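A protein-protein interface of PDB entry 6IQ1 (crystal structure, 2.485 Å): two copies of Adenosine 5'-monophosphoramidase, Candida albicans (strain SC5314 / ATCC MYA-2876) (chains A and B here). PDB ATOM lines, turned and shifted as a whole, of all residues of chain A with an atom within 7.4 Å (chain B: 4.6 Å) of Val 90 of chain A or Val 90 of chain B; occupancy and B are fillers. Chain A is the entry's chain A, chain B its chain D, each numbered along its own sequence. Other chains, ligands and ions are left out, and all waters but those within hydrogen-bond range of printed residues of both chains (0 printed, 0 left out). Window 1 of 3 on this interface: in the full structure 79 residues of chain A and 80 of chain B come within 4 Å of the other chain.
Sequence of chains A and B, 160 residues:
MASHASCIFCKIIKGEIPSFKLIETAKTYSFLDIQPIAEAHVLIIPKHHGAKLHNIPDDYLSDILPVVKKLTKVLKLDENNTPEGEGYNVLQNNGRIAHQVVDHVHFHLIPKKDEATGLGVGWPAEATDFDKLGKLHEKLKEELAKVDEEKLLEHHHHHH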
ATOM      1  N   ILE A  44      -4.403 -24.411   4.880  1.00  0.00           N
ATOM      2  CA  ILE A  44      -5.238 -23.252   4.554  1.00  0.00           C
ATOM      3  C   ILE A  44      -4.403 -22.283   3.724  1.00  0.00           C
ATOM      4  O   ILE A  44      -3.368 -21.790   4.189  1.00  0.00           O
ATOM      5  CB  ILE A  44      -5.767 -22.554   5.815  1.00  0.00           C
ATOM      6  CG1 ILE A  44      -6.412 -23.567   6.767  1.00  0.00           C
ATOM      7  CG2 ILE A  44      -6.731 -21.467   5.451  1.00  0.00           C
ATOM      8  CD1 ILE A  44      -5.457 -24.125   7.849  1.00  0.00           C
ATOM      9  N   LEU A  53       4.854 -14.922   3.288  1.00  0.00           N
ATOM     10  CA  LEU A  53       3.770 -14.167   3.904  1.00  0.00           C
ATOM     11  C   LEU A  53       3.735 -12.735   3.389  1.00  0.00           C
ATOM     12  O   LEU A  53       2.663 -12.197   3.074  1.00  0.00           O
ATOM     13  CB  LEU A  53       3.912 -14.176   5.428  1.00  0.00           C
ATOM     14  CG  LEU A  53       2.682 -13.601   6.145  1.00  0.00           C
ATOM     15  CD1 LEU A  53       1.600 -14.683   6.278  1.00  0.00           C
ATOM     16  CD2 LEU A  53       3.033 -12.986   7.503  1.00  0.00           C
ATOM     17  N   ILE A  64      -7.608 -15.372   6.439  1.00  0.00           N
ATOM     18  CA  ILE A  64      -7.054 -16.686   6.738  1.00  0.00           C
ATOM     19  C   ILE A  64      -7.431 -17.142   8.152  1.00  0.00           C
ATOM     20  O   ILE A  64      -7.976 -18.239   8.335  1.00  0.00           O
ATOM     21  CB  ILE A  64      -5.535 -16.686   6.505  1.00  0.00           C
ATOM     22  CG1 ILE A  64      -5.262 -16.721   5.002  1.00  0.00           C
ATOM     23  CG2 ILE A  64      -4.892 -17.883   7.181  1.00  0.00           C
ATOM     24  CD1 ILE A  64      -3.846 -16.433   4.661  1.00  0.00           C
ATOM     25  N   LEU A  65      -7.137 -16.338   9.174  1.00  0.00           N
ATOM     26  CA  LEU A  65      -7.438 -16.796  10.532  1.00  0.00           C
ATOM     27  C   LEU A  65      -8.932 -17.013  10.790  1.00  0.00           C
ATOM     28  O   LEU A  65      -9.263 -18.001  11.465  1.00  0.00           O
ATOM     29  CB  LEU A  65      -6.840 -15.842  11.571  1.00  0.00           C
ATOM     30  CG  LEU A  65      -5.320 -15.758  11.500  1.00  0.00           C
ATOM     31  CD1 LEU A  65      -4.805 -14.907  12.621  1.00  0.00           C
ATOM     32  CD2 LEU A  65      -4.712 -17.139  11.541  1.00  0.00           C
ATOM     33  N   VAL A  68      -9.322 -20.403   9.573  1.00  0.00           N
ATOM     34  CA  VAL A  68      -8.674 -21.350  10.479  1.00  0.00           C
ATOM     35  C   VAL A  68      -9.539 -21.558  11.717  1.00  0.00           C
ATOM     36  O   VAL A  68      -9.767 -22.693  12.152  1.00  0.00           O
ATOM     37  CB  VAL A  68      -7.250 -20.881  10.848  1.00  0.00           C
ATOM     38  CG1 VAL A  68      -6.647 -21.783  11.905  1.00  0.00           C
ATOM     39  CG2 VAL A  68      -6.342 -20.842   9.628  1.00  0.00           C
ATOM     40  N   LYS A  69     -10.073 -20.468  12.278  1.00  0.00           N
ATOM     41  CA  LYS A  69     -10.864 -20.593  13.502  1.00  0.00           C
ATOM     42  C   LYS A  69     -12.135 -21.399  13.250  1.00  0.00           C
ATOM     43  O   LYS A  69     -12.533 -22.231  14.081  1.00  0.00           O
ATOM     44  CB  LYS A  69     -11.202 -19.212  14.064  1.00  0.00           C
ATOM     45  CG  LYS A  69     -12.340 -19.203  15.069  1.00  0.00           C
ATOM     46  CD  LYS A  69     -12.892 -17.798  15.209  1.00  0.00           C
ATOM     47  CE  LYS A  69     -14.077 -17.748  16.154  1.00  0.00           C
ATOM     48  NZ  LYS A  69     -14.523 -16.330  16.403  1.00  0.00           N
ATOM     49  N   THR A  72     -11.421 -24.971  13.332  1.00  0.00           N
ATOM     50  CA  THR A  72     -11.326 -25.564  14.668  1.00  0.00           C
ATOM     51  C   THR A  72     -12.695 -25.980  15.203  1.00  0.00           C
ATOM     52  O   THR A  72     -12.791 -26.937  15.985  1.00  0.00           O
ATOM     53  CB  THR A  72     -10.647 -24.620  15.660  1.00  0.00           C
ATOM     54  OG1 THR A  72     -11.554 -23.587  16.056  1.00  0.00           O
ATOM     55  CG2 THR A  72      -9.421 -24.005  15.043  1.00  0.00           C
ATOM     56  N   TYR A  88      -3.544 -27.632  19.894  1.00  0.00           N
ATOM     57  CA  TYR A  88      -3.266 -27.553  18.469  1.00  0.00           C
ATOM     58  C   TYR A  88      -2.333 -26.388  18.197  1.00  0.00           C
ATOM     59  O   TYR A  88      -2.217 -25.454  18.994  1.00  0.00           O
ATOM     60  CB  TYR A  88      -4.553 -27.422  17.628  1.00  0.00           C
ATOM     61  CG  TYR A  88      -5.464 -26.262  17.946  1.00  0.00           C
ATOM     62  CD1 TYR A  88      -6.351 -26.321  19.025  1.00  0.00           C
ATOM     63  CD2 TYR A  88      -5.478 -25.121  17.143  1.00  0.00           C
ATOM     64  CE1 TYR A  88      -7.203 -25.274  19.312  1.00  0.00           C
ATOM     65  CE2 TYR A  88      -6.341 -24.055  17.421  1.00  0.00           C
ATOM     66  CZ  TYR A  88      -7.198 -24.147  18.504  1.00  0.00           C
ATOM     67  OH  TYR A  88      -8.047 -23.111  18.799  1.00  0.00           O
ATOM     68  N   ASN A  89      -1.669 -26.458  17.050  1.00  0.00           N
ATOM     69  CA  ASN A  89      -0.755 -25.420  16.623  1.00  0.00           C
ATOM     70  C   ASN A  89      -1.205 -24.855  15.286  1.00  0.00           C
ATOM     71  O   ASN A  89      -1.829 -25.545  14.470  1.00  0.00           O
ATOM     72  CB  ASN A  89       0.662 -25.953  16.484  1.00  0.00           C
ATOM     73  CG  ASN A  89       1.238 -26.446  17.797  1.00  0.00           C
ATOM     74  OD1 ASN A  89       1.173 -27.644  18.107  1.00  0.00           O
ATOM     75  ND2 ASN A  89       1.831 -25.532  18.563  1.00  0.00           N
ATOM     76  N   VAL A  90      -0.888 -23.586  15.076  1.00  0.00           N
ATOM     77  CA  VAL A  90      -1.007 -22.936  13.781  1.00  0.00           C
ATOM     78  C   VAL A  90       0.394 -22.496  13.393  1.00  0.00           C
ATOM     79  O   VAL A  90       1.085 -21.839  14.184  1.00  0.00           O
ATOM     80  CB  VAL A  90      -1.977 -21.737  13.824  1.00  0.00           C
ATOM     81  CG1 VAL A  90      -2.067 -21.074  12.479  1.00  0.00           C
ATOM     82  CG2 VAL A  90      -3.334 -22.176  14.312  1.00  0.00           C
ATOM     83  N   LEU A  91       0.825 -22.891  12.195  1.00  0.00           N
ATOM     84  CA  LEU A  91       2.204 -22.690  11.777  1.00  0.00           C
ATOM     85  C   LEU A  91       2.229 -22.323  10.304  1.00  0.00           C
ATOM     86  O   LEU A  91       1.513 -22.918   9.495  1.00  0.00           O
ATOM     87  CB  LEU A  91       3.052 -23.956  12.030  1.00  0.00           C
ATOM     88  CG  LEU A  91       4.476 -23.999  11.468  1.00  0.00           C
ATOM     89  CD1 LEU A  91       5.411 -23.173  12.336  1.00  0.00           C
ATOM     90  CD2 LEU A  91       4.961 -25.430  11.367  1.00  0.00           C
ATOM     91  N   GLN A  92       3.058 -21.345   9.970  1.00  0.00           N
ATOM     92  CA  GLN A  92       3.292 -20.949   8.594  1.00  0.00           C
ATOM     93  C   GLN A  92       4.790 -20.758   8.414  1.00  0.00           C
ATOM     94  O   GLN A  92       5.439 -20.142   9.266  1.00  0.00           O
ATOM     95  CB  GLN A  92       2.520 -19.670   8.246  1.00  0.00           C
ATOM     96  CG  GLN A  92       2.451 -19.376   6.756  1.00  0.00           C
ATOM     97  CD  GLN A  92       3.525 -18.415   6.308  1.00  0.00           C
ATOM     98  OE1 GLN A  92       3.931 -17.529   7.070  1.00  0.00           O
ATOM     99  NE2 GLN A  92       3.994 -18.573   5.070  1.00  0.00           N
ATOM    100  N   ASN A  93       5.331 -21.287   7.312  1.00  0.00           N
ATOM    101  CA  ASN A  93       6.768 -21.340   7.080  1.00  0.00           C
ATOM    102  C   ASN A  93       7.167 -20.535   5.846  1.00  0.00           C
ATOM    103  O   ASN A  93       6.454 -20.512   4.834  1.00  0.00           O
ATOM    104  CB  ASN A  93       7.252 -22.793   6.930  1.00  0.00           C
ATOM    105  CG  ASN A  93       6.882 -23.663   8.127  1.00  0.00           C
ATOM    106  OD1 ASN A  93       6.803 -23.199   9.265  1.00  0.00           O
ATOM    107  ND2 ASN A  93       6.665 -24.940   7.865  1.00  0.00           N
ATOM    108  N   ASN A  94       8.339 -19.909   5.934  1.00  0.00           N
ATOM    109  CA  ASN A  94       8.818 -18.977   4.917  1.00  0.00           C
ATOM    110  C   ASN A  94      10.294 -19.285   4.675  1.00  0.00           C
ATOM    111  O   ASN A  94      11.159 -18.896   5.469  1.00  0.00           O
ATOM    112  CB  ASN A  94       8.600 -17.525   5.351  1.00  0.00           C
ATOM    113  CG  ASN A  94       7.137 -17.219   5.643  1.00  0.00           C
ATOM    114  OD1 ASN A  94       6.381 -16.858   4.745  1.00  0.00           O
ATOM    115  ND2 ASN A  94       6.734 -17.359   6.906  1.00  0.00           N
ATOM    116  N   ALA A  98      13.411 -22.437   6.999  1.00  0.00           N
ATOM    117  CA  ALA A  98      12.297 -22.416   7.936  1.00  0.00           C
ATOM    118  C   ALA A  98      11.277 -23.531   7.686  1.00  0.00           C
ATOM    119  O   ALA A  98      10.181 -23.470   8.257  1.00  0.00           O
ATOM    120  CB  ALA A  98      11.601 -21.055   7.890  1.00  0.00           C
ATOM    121  N   PHE A 107      -0.868 -22.109   5.699  1.00  0.00           N
ATOM    122  CA  PHE A 107      -0.923 -22.274   7.143  1.00  0.00           C
ATOM    123  C   PHE A 107      -1.307 -23.707   7.480  1.00  0.00           C
ATOM    124  O   PHE A 107      -2.262 -24.245   6.909  1.00  0.00           O
ATOM    125  CB  PHE A 107      -1.943 -21.311   7.741  1.00  0.00           C
ATOM    126  CG  PHE A 107      -1.470 -19.895   7.797  1.00  0.00           C
ATOM    127  CD1 PHE A 107      -1.458 -19.109   6.655  1.00  0.00           C
ATOM    128  CD2 PHE A 107      -1.043 -19.344   8.998  1.00  0.00           C
ATOM    129  CE1 PHE A 107      -1.022 -17.805   6.716  1.00  0.00           C
ATOM    130  CE2 PHE A 107      -0.615 -18.050   9.062  1.00  0.00           C
ATOM    131  CZ  PHE A 107      -0.603 -17.276   7.922  1.00  0.00           C
ATOM    132  N   HIS A 108      -0.555 -24.321   8.392  1.00  0.00           N
ATOM    133  CA  HIS A 108      -0.886 -25.628   8.946  1.00  0.00           C
ATOM    134  C   HIS A 108      -1.738 -25.455  10.204  1.00  0.00           C
ATOM    135  O   HIS A 108      -1.323 -24.766  11.144  1.00  0.00           O
ATOM    136  CB  HIS A 108       0.378 -26.416   9.319  1.00  0.00           C
ATOM    137  CG  HIS A 108       1.399 -26.545   8.228  1.00  0.00           C
ATOM    138  ND1 HIS A 108       1.551 -27.701   7.487  1.00  0.00           N
ATOM    139  CD2 HIS A 108       2.360 -25.692   7.795  1.00  0.00           C
ATOM    140  CE1 HIS A 108       2.541 -27.541   6.625  1.00  0.00           C
ATOM    141  NE2 HIS A 108       3.046 -26.330   6.785  1.00  0.00           N
ATOM    142  N   LEU A 109      -2.916 -26.091  10.229  1.00  0.00           N
ATOM    143  CA  LEU A 109      -3.670 -26.327  11.461  1.00  0.00           C
ATOM    144  C   LEU A 109      -3.416 -27.767  11.923  1.00  0.00           C
ATOM    145  O   LEU A 109      -3.927 -28.719  11.320  1.00  0.00           O
ATOM    146  CB  LEU A 109      -5.162 -26.087  11.263  1.00  0.00           C
ATOM    147  CG  LEU A 109      -6.014 -26.459  12.488  1.00  0.00           C
ATOM    148  CD1 LEU A 109      -5.575 -25.691  13.730  1.00  0.00           C
ATOM    149  CD2 LEU A 109      -7.491 -26.208  12.214  1.00  0.00           C
ATOM    150  N   ILE A 110      -2.638 -27.929  12.988  1.00  0.00           N
ATOM    151  CA  ILE A 110      -2.172 -29.260  13.380  1.00  0.00           C
ATOM    152  C   ILE A 110      -2.675 -29.599  14.779  1.00  0.00           C
ATOM    153  O   ILE A 110      -2.227 -28.994  15.768  1.00  0.00           O
ATOM    154  CB  ILE A 110      -0.634 -29.360  13.326  1.00  0.00           C
ATOM    155  CG1 ILE A 110      -0.079 -28.765  12.036  1.00  0.00           C
ATOM    156  CG2 ILE A 110      -0.177 -30.792  13.479  1.00  0.00           C
ATOM    157  CD1 ILE A 110       1.412 -28.592  12.090  1.00  0.00           C
ATOM    158  N   LEU A 119       2.877 -31.214  15.931  1.00  0.00           N
ATOM    159  CA  LEU A 119       4.095 -30.418  15.870  1.00  0.00           C
ATOM    160  C   LEU A 119       4.979 -30.677  17.089  1.00  0.00           C
ATOM    161  O   LEU A 119       4.493 -30.812  18.217  1.00  0.00           O
ATOM    162  CB  LEU A 119       3.748 -28.931  15.790  1.00  0.00           C
ATOM    163  CG  LEU A 119       4.926 -28.006  15.536  1.00  0.00           C
ATOM    164  CD1 LEU A 119       5.510 -28.252  14.127  1.00  0.00           C
ATOM    165  CD2 LEU A 119       4.492 -26.560  15.727  1.00  0.00           C
ATOM    166  N   LEU B  53      -7.115 -19.712  19.977  1.00  0.00           N
ATOM    167  CA  LEU B  53      -7.500 -19.072  18.723  1.00  0.00           C
ATOM    168  C   LEU B  53      -9.019 -19.003  18.561  1.00  0.00           C
ATOM    169  O   LEU B  53      -9.558 -17.989  18.112  1.00  0.00           O
ATOM    170  CB  LEU B  53      -6.875 -19.809  17.540  1.00  0.00           C
ATOM    171  CG  LEU B  53      -6.967 -19.026  16.230  1.00  0.00           C
ATOM    172  CD1 LEU B  53      -5.848 -18.002  16.182  1.00  0.00           C
ATOM    173  CD2 LEU B  53      -6.932 -19.925  15.014  1.00  0.00           C
ATOM    174  N   VAL B  68       1.422  -8.746  11.208  1.00  0.00           N
ATOM    175  CA  VAL B  68       2.620  -9.578  11.071  1.00  0.00           C
ATOM    176  C   VAL B  68       3.330  -9.251   9.763  1.00  0.00           C
ATOM    177  O   VAL B  68       4.557  -9.122   9.716  1.00  0.00           O
ATOM    178  CB  VAL B  68       2.271 -11.080  11.169  1.00  0.00           C
ATOM    179  CG1 VAL B  68       3.522 -11.941  11.027  1.00  0.00           C
ATOM    180  CG2 VAL B  68       1.569 -11.397  12.478  1.00  0.00           C
ATOM    181  N   TYR B  88      11.695 -17.355   8.032  1.00  0.00           N
ATOM    182  CA  TYR B  88      10.974 -17.039   9.260  1.00  0.00           C
ATOM    183  C   TYR B  88       9.741 -17.929   9.404  1.00  0.00           C
ATOM    184  O   TYR B  88       9.229 -18.495   8.429  1.00  0.00           O
ATOM    185  CB  TYR B  88      10.581 -15.549   9.340  1.00  0.00           C
ATOM    186  CG  TYR B  88       9.711 -14.985   8.228  1.00  0.00           C
ATOM    187  CD1 TYR B  88      10.278 -14.487   7.057  1.00  0.00           C
ATOM    188  CD2 TYR B  88       8.330 -14.895   8.376  1.00  0.00           C
ATOM    189  CE1 TYR B  88       9.495 -13.948   6.048  1.00  0.00           C
ATOM    190  CE2 TYR B  88       7.534 -14.338   7.383  1.00  0.00           C
ATOM    191  CZ  TYR B  88       8.120 -13.869   6.217  1.00  0.00           C
ATOM    192  OH  TYR B  88       7.330 -13.341   5.217  1.00  0.00           O
ATOM    193  N   ASN B  89       9.281 -18.043  10.652  1.00  0.00           N
ATOM    194  CA  ASN B  89       8.123 -18.844  11.018  1.00  0.00           C
ATOM    195  C   ASN B  89       7.075 -17.989  11.728  1.00  0.00           C
ATOM    196  O   ASN B  89       7.407 -17.077  12.494  1.00  0.00           O
ATOM    197  CB  ASN B  89       8.536 -20.007  11.912  1.00  0.00           C
ATOM    198  CG  ASN B  89       9.391 -21.016  11.179  1.00  0.00           C
ATOM    199  OD1 ASN B  89      10.626 -20.971  11.256  1.00  0.00           O
ATOM    200  ND2 ASN B  89       8.738 -21.934  10.442  1.00  0.00           N
ATOM    201  N   VAL B  90       5.805 -18.288  11.467  1.00  0.00           N
ATOM    202  CA  VAL B  90       4.695 -17.748  12.243  1.00  0.00           C
ATOM    203  C   VAL B  90       4.101 -18.915  13.020  1.00  0.00           C
ATOM    204  O   VAL B  90       3.679 -19.912  12.422  1.00  0.00           O
ATOM    205  CB  VAL B  90       3.657 -17.052  11.346  1.00  0.00           C
ATOM    206  CG1 VAL B  90       2.584 -16.320  12.188  1.00  0.00           C
ATOM    207  CG2 VAL B  90       4.353 -16.055  10.424  1.00  0.00           C
ATOM    208  N   LEU B  91       4.111 -18.819  14.354  1.00  0.00           N
ATOM    209  CA  LEU B  91       3.635 -19.903  15.205  1.00  0.00           C
ATOM    210  C   LEU B  91       2.603 -19.393  16.206  1.00  0.00           C
ATOM    211  O   LEU B  91       2.756 -18.306  16.776  1.00  0.00           O
ATOM    212  CB  LEU B  91       4.791 -20.553  15.955  1.00  0.00           C
ATOM    213  CG  LEU B  91       4.438 -21.720  16.882  1.00  0.00           C
ATOM    214  CD1 LEU B  91       3.804 -22.830  16.080  1.00  0.00           C
ATOM    215  CD2 LEU B  91       5.688 -22.218  17.621  1.00  0.00           C
ATOM    216  N   GLN B  92       1.554 -20.184  16.416  1.00  0.00           N
ATOM    217  CA  GLN B  92       0.537 -19.902  17.424  1.00  0.00           C
ATOM    218  C   GLN B  92       0.172 -21.212  18.107  1.00  0.00           C
ATOM    219  O   GLN B  92      -0.101 -22.205  17.423  1.00  0.00           O
ATOM    220  CB  GLN B  92      -0.708 -19.252  16.801  1.00  0.00           C
ATOM    221  CG  GLN B  92      -1.581 -18.520  17.807  1.00  0.00           C
ATOM    222  CD  GLN B  92      -2.738 -19.361  18.271  1.00  0.00           C
ATOM    223  OE1 GLN B  92      -3.248 -20.179  17.510  1.00  0.00           O
ATOM    224  NE2 GLN B  92      -3.156 -19.181  19.520  1.00  0.00           N
ATOM    225  N   PHE B 107       0.788 -14.637  18.724  1.00  0.00           N
ATOM    226  CA  PHE B 107       1.478 -15.141  17.555  1.00  0.00           C
ATOM    227  C   PHE B 107       2.963 -14.827  17.671  1.00  0.00           C
ATOM    228  O   PHE B 107       3.341 -13.735  18.107  1.00  0.00           O
ATOM    229  CB  PHE B 107       0.877 -14.502  16.293  1.00  0.00           C
ATOM    230  CG  PHE B 107      -0.456 -15.080  15.905  1.00  0.00           C
ATOM    231  CD1 PHE B 107      -1.615 -14.648  16.518  1.00  0.00           C
ATOM    232  CD2 PHE B 107      -0.544 -16.075  14.934  1.00  0.00           C
ATOM    233  CE1 PHE B 107      -2.846 -15.192  16.168  1.00  0.00           C
ATOM    234  CE2 PHE B 107      -1.762 -16.617  14.574  1.00  0.00           C
ATOM    235  CZ  PHE B 107      -2.912 -16.187  15.193  1.00  0.00           C
ATOM    236  N   HIS B 108       3.806 -15.778  17.287  1.00  0.00           N
ATOM    237  CA  HIS B 108       5.248 -15.558  17.235  1.00  0.00           C
ATOM    238  C   HIS B 108       5.671 -15.290  15.792  1.00  0.00           C
ATOM    239  O   HIS B 108       5.351 -16.074  14.885  1.00  0.00           O
ATOM    240  CB  HIS B 108       6.036 -16.765  17.762  1.00  0.00           C
ATOM    241  CG  HIS B 108       5.679 -17.191  19.152  1.00  0.00           C
ATOM    242  ND1 HIS B 108       6.396 -16.792  20.261  1.00  0.00           N
ATOM    243  CD2 HIS B 108       4.691 -17.996  19.610  1.00  0.00           C
ATOM    244  CE1 HIS B 108       5.856 -17.326  21.343  1.00  0.00           C
ATOM    245  NE2 HIS B 108       4.817 -18.057  20.976  1.00  0.00           N
ATOM    246  N   LEU B 109       6.398 -14.200  15.582  1.00  0.00           N
ATOM    247  CA  LEU B 109       7.109 -13.950  14.329  1.00  0.00           C
ATOM    248  C   LEU B 109       8.582 -14.217  14.612  1.00  0.00           C
ATOM    249  O   LEU B 109       9.230 -13.437  15.318  1.00  0.00           O
ATOM    250  CB  LEU B 109       6.892 -12.524  13.824  1.00  0.00           C
ATOM    251  CG  LEU B 109       7.823 -12.163  12.660  1.00  0.00           C
ATOM    252  CD1 LEU B 109       7.633 -13.122  11.484  1.00  0.00           C
ATOM    253  CD2 LEU B 109       7.636 -10.741  12.197  1.00  0.00           C
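Of the printed residues of chain B, Val 90 of chain A touches Val 90 (3.7 Å), Leu 91 (3.4 Å) and Gln 92 (2.8 Å).
Of the printed residues of chain A, Val 90 of chain B touches Val 90, Leu 91 and Gln 92.
Printed residues of chain A within 4 Å of Val 68 of chain B: Leu 53.
Of the printed residues of chain B, Tyr 88 of chain A touches Leu 53.
The nearest printed residue of chain A that does not touch Val 90 of chain B is Leu 53 of chain A (4.4 Å).
Among the printed residues, merely in contact across the chains: Leu 53 of chain A with Val 68 of chain B (3.7 Å), Leu 53 of chain A with Tyr 88 of chain B (3.5 Å), Leu 65 of chain A with Phe 107 of chain B (3.4 Å), Val 68 of chain A with Leu 53 of chain B (3.6 Å), Tyr 88 of chain A with Leu 53 of chain B (3.7 Å), Asn 89 of chain A with Gln 92 of chain B (3.4 Å), Val 90 of chain A with Val 90 of chain B (3.7 Å), Val 90 of chain A with Leu 91 of chain B (3.4 Å), Leu 91 of chain A with Val 90 of chain B (3.2 Å), Gln 92 of chain A with Asn 89 of chain B (3.5 Å), Asn 93 of chain A with Tyr 88 of chain B (3.9 Å), Ala 98 of chain A with Tyr 88 of chain B (3.5 Å) and Leu 119 of chain A with Leu 91 of chain B (3.8 Å).
The side-chain amide oxygen of Asn 94 of chain A lies within hydrogen-bond range of the backbone NH of Leu 53 of chain A, at 2.9 Å.
The backbone NH (N) of Asn 89 of chain A sits at hydrogen-bond distance from the backbone carbonyl oxygen (O) of Ile 110 of chain A (2.9 Å).
N of His 108 of chain A lies within hydrogen-bond range of O of Leu 91 of chain A (2.7 Å).
OE1 of Gln 92 of chain A sits at hydrogen-bond distance from ND2 of Asn 94 of chain A.
O of Leu 91 of chain B lies within hydrogen-bond range of N of His 108 of chain B.
O of Val 90 of chain A sits at hydrogen-bond distance from N of Gln 92 of chain B (2.8 Å).
The backbone carbonyl oxygen of Gln 92 of chain A sits at hydrogen-bond distance from the backbone NH of Val 90 of chain B (2.9 Å).
OD1 of Asn 93 of chain A sits at hydrogen-bond distance from ND2 of Asn 89 of chain B.
O of Tyr 88 of chain B sits at hydrogen-bond distance from N of Asn 94 of chain A (3.0 Å).
O of Ala 98 of chain A lies within hydrogen-bond range of ND2 of Asn 89 of chain B, 3.0 Å away.
Hydrophobic or aromatic side chains of chain A within 4 Å of the printed part of chain B: Leu 53, Leu 65, Val 68, Tyr 88, Val 90, Leu 91, Ala 98 and Leu 119.
Along chain A the printed residues that touch a printed residue of chain B span positions 53 to 119.
Of the 10 printed residues of chain B, 8 touch a printed residue of chain A.
Hydrophobic or aromatic side chains of chain B that line the printed part of chain A: Leu 53, Val 68, Tyr 88, Val 90, Leu 91 and Phe 107.
Among the printed residues, 18 pairs touch across the chains.
Leu 53 of chain A touches Val 68 of chain B, and with the chains exchanged Val 68 of chain A touches Leu 53 of chain B.
Leu 53 of chain A touches Tyr 88 of chain B, and with the chains exchanged Tyr 88 of chain A touches Leu 53 of chain B.
Asn 89 of chain A touches Gln 92 of chain B, and with the chains exchanged Gln 92 of chain A touches Asn 89 of chain B.
Val 90 of chain A touches Leu 91 of chain B, and with the chains exchanged Leu 91 of chain A touches Val 90 of chain B.
Of the 18 pairs that touch across the chains among the printed residues, 11 have their exchanged pair printed and touching as well.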
